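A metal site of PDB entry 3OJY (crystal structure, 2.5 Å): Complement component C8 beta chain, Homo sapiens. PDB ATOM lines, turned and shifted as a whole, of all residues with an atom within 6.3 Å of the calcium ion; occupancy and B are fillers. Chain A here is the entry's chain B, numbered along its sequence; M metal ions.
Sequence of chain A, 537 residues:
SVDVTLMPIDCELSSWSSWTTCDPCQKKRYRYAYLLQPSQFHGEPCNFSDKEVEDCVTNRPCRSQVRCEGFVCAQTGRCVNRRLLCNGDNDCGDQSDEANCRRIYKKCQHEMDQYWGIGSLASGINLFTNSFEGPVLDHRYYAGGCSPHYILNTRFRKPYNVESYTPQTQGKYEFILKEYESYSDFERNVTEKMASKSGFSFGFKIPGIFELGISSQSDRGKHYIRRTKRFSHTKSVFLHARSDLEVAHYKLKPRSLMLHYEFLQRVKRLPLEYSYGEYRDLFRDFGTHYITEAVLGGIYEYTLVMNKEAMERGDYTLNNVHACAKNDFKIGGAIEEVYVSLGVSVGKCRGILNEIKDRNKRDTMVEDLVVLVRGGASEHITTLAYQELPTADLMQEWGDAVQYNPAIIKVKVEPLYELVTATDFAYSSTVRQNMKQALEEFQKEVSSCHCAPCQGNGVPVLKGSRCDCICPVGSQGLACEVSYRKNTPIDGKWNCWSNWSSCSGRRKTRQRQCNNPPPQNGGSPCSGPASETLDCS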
ATOM      1  N   LEU A  84     -14.758 -13.362 -21.419  1.00  0.00           N
ATOM      2  CA  LEU A  84     -15.878 -13.125 -22.350  1.00  0.00           C
ATOM      3  C   LEU A  84     -16.802 -11.958 -22.011  1.00  0.00           C
ATOM      4  O   LEU A  84     -17.741 -11.668 -22.756  1.00  0.00           O
ATOM      5  CB  LEU A  84     -16.689 -14.413 -22.607  1.00  0.00           C
ATOM      6  CG  LEU A  84     -15.837 -15.587 -23.149  1.00  0.00           C
ATOM      7  CD1 LEU A  84     -16.675 -16.765 -23.514  1.00  0.00           C
ATOM      8  CD2 LEU A  84     -14.921 -15.175 -24.319  1.00  0.00           C
ATOM      9  N   LEU A  85     -16.561 -11.290 -20.891  1.00  0.00           N
ATOM     10  CA  LEU A  85     -17.320 -10.090 -20.572  1.00  0.00           C
ATOM     11  C   LEU A  85     -16.897  -8.957 -21.482  1.00  0.00           C
ATOM     12  O   LEU A  85     -15.702  -8.802 -21.741  1.00  0.00           O
ATOM     13  CB  LEU A  85     -17.119  -9.705 -19.129  1.00  0.00           C
ATOM     14  CG  LEU A  85     -17.761 -10.552 -18.028  1.00  0.00           C
ATOM     15  CD1 LEU A  85     -17.490  -9.864 -16.687  1.00  0.00           C
ATOM     16  CD2 LEU A  85     -19.242 -10.721 -18.243  1.00  0.00           C
ATOM     17  N   CYS A  86     -17.857  -8.171 -21.962  1.00  0.00           N
ATOM     18  CA  CYS A  86     -17.621  -7.022 -22.858  1.00  0.00           C
ATOM     19  C   CYS A  86     -16.733  -7.305 -24.096  1.00  0.00           C
ATOM     20  O   CYS A  86     -15.786  -6.560 -24.379  1.00  0.00           O
ATOM     21  CB  CYS A  86     -17.074  -5.803 -22.079  1.00  0.00           C
ATOM     22  SG  CYS A  86     -17.862  -5.459 -20.535  1.00  0.00           S
ATOM     23  N   ASN A  87     -17.038  -8.379 -24.819  1.00  0.00           N
ATOM     24  CA  ASN A  87     -16.417  -8.651 -26.088  1.00  0.00           C
ATOM     25  C   ASN A  87     -17.391  -8.488 -27.300  1.00  0.00           C
ATOM     26  O   ASN A  87     -17.108  -8.951 -28.411  1.00  0.00           O
ATOM     27  CB  ASN A  87     -15.809 -10.040 -26.053  1.00  0.00           C
ATOM     28  CG  ASN A  87     -16.850 -11.129 -25.969  1.00  0.00           C
ATOM     29  OD1 ASN A  87     -18.012 -10.857 -25.683  1.00  0.00           O
ATOM     30  ND2 ASN A  87     -16.430 -12.379 -26.207  1.00  0.00           N
ATOM     31  N   GLY A  88     -18.532  -7.851 -27.078  1.00  0.00           N
ATOM     32  CA  GLY A  88     -19.519  -7.695 -28.140  1.00  0.00           C
ATOM     33  C   GLY A  88     -20.205  -8.985 -28.611  1.00  0.00           C
ATOM     34  O   GLY A  88     -20.963  -8.963 -29.579  1.00  0.00           O
ATOM     35  N   ASP A  89     -19.942 -10.092 -27.913  1.00  0.00           N
ATOM     36  CA  ASP A  89     -20.641 -11.359 -28.146  1.00  0.00           C
ATOM     37  C   ASP A  89     -21.629 -11.570 -27.037  1.00  0.00           C
ATOM     38  O   ASP A  89     -21.451 -11.080 -25.931  1.00  0.00           O
ATOM     39  CB  ASP A  89     -19.666 -12.534 -28.076  1.00  0.00           C
ATOM     40  CG  ASP A  89     -18.772 -12.627 -29.282  1.00  0.00           C
ATOM     41  OD1 ASP A  89     -17.736 -13.337 -29.233  1.00  0.00           O
ATOM     42  OD2 ASP A  89     -19.147 -11.995 -30.305  1.00  0.00           O
ATOM     43  N   ASN A  90     -22.673 -12.336 -27.319  1.00  0.00           N
ATOM     44  CA  ASN A  90     -23.577 -12.783 -26.282  1.00  0.00           C
ATOM     45  C   ASN A  90     -23.211 -14.208 -25.900  1.00  0.00           C
ATOM     46  O   ASN A  90     -23.730 -15.164 -26.462  1.00  0.00           O
ATOM     47  CB  ASN A  90     -25.018 -12.695 -26.759  1.00  0.00           C
ATOM     48  CG  ASN A  90     -25.975 -12.470 -25.622  1.00  0.00           C
ATOM     49  OD1 ASN A  90     -25.724 -12.868 -24.468  1.00  0.00           O
ATOM     50  ND2 ASN A  90     -27.100 -11.835 -25.929  1.00  0.00           N
ATOM     51  N   ASP A  91     -22.278 -14.327 -24.960  1.00  0.00           N
ATOM     52  CA  ASP A  91     -21.749 -15.624 -24.554  1.00  0.00           C
ATOM     53  C   ASP A  91     -22.666 -16.237 -23.483  1.00  0.00           C
ATOM     54  O   ASP A  91     -22.870 -17.464 -23.430  1.00  0.00           O
ATOM     55  CB  ASP A  91     -20.320 -15.477 -24.009  1.00  0.00           C
ATOM     56  CG  ASP A  91     -19.377 -14.817 -25.006  1.00  0.00           C
ATOM     57  OD1 ASP A  91     -18.897 -15.555 -25.880  1.00  0.00           O
ATOM     58  OD2 ASP A  91     -19.123 -13.581 -24.905  1.00  0.00           O
ATOM     59  N   CYS A  92     -23.247 -15.386 -22.648  1.00  0.00           N
ATOM     60  CA  CYS A  92     -24.221 -15.882 -21.697  1.00  0.00           C
ATOM     61  C   CYS A  92     -25.367 -16.426 -22.470  1.00  0.00           C
ATOM     62  O   CYS A  92     -26.272 -17.054 -21.907  1.00  0.00           O
ATOM     63  CB  CYS A  92     -24.691 -14.796 -20.753  1.00  0.00           C
ATOM     64  SG  CYS A  92     -23.570 -14.834 -19.411  1.00  0.00           S
ATOM     65  N   ASP A  97     -23.312 -11.140 -20.479  1.00  0.00           N
ATOM     66  CA  ASP A  97     -21.923 -10.854 -20.239  1.00  0.00           C
ATOM     67  C   ASP A  97     -21.634  -9.423 -20.768  1.00  0.00           C
ATOM     68  O   ASP A  97     -20.535  -8.918 -20.630  1.00  0.00           O
ATOM     69  CB  ASP A  97     -21.061 -11.906 -20.961  1.00  0.00           C
ATOM     70  CG  ASP A  97     -21.666 -12.339 -22.327  1.00  0.00           C
ATOM     71  OD1 ASP A  97     -20.889 -12.535 -23.279  1.00  0.00           O
ATOM     72  OD2 ASP A  97     -22.891 -12.465 -22.455  1.00  0.00           O
ATOM     73  N   GLU A  98     -22.639  -8.756 -21.328  1.00  0.00           N
ATOM     74  CA  GLU A  98     -22.452  -7.506 -22.083  1.00  0.00           C
ATOM     75  C   GLU A  98     -23.151  -6.279 -21.488  1.00  0.00           C
ATOM     76  O   GLU A  98     -23.185  -5.209 -22.140  1.00  0.00           O
ATOM     77  CB  GLU A  98     -22.914  -7.699 -23.540  1.00  0.00           C
ATOM     78  CG  GLU A  98     -22.141  -8.745 -24.328  1.00  0.00           C
ATOM     79  CD  GLU A  98     -20.604  -8.501 -24.371  1.00  0.00           C
ATOM     80  OE1 GLU A  98     -20.209  -7.380 -24.725  1.00  0.00           O
ATOM     81  OE2 GLU A  98     -19.806  -9.446 -24.097  1.00  0.00           O
HETATM   82 CA    CA M   1     -19.482 -11.365 -24.253  1.00  0.00          CA
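Of the 11 residues printed, 6 come within 4 Å of the calcium ion.
The nearest printed residue that does not touch the calcium ion is Cys 86 (4.3 Å).
The side-chain amide oxygen (OD1) of Asn 90 sits close to the side-chain carboxylate (OD2) of Asp 97 (3.5 Å).
O of Asp 97 lies within hydrogen-bond range of N of Cys 86 (3.1 Å).
OE1 of Glu 98 is in hydrogen-bond range of N of Gly 88 (2.9 Å).
N of Cys 92 lies within hydrogen-bond range of OD2 of Asp 97 (2.9 Å).
N of Cys 86 sits close to OE2 of Glu 98 (3.2 Å).
The calcium ion is bound by OE2 of Glu 98, at 2.0 Å.
The calcium ion is bound by the side-chain carboxylate (OD1) of Asp 97 (2.1 Å).
The calcium ion is bound by OD1 of Asn 87 (2.1 Å).
O of Leu 84 binds the calcium ion (2.3 Å).
The calcium ion is bound by the side-chain carboxylate (OD2) of Asp 91, at 2.3 Å.
O of Asp 89 is bound to the calcium ion (2.6 Å).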
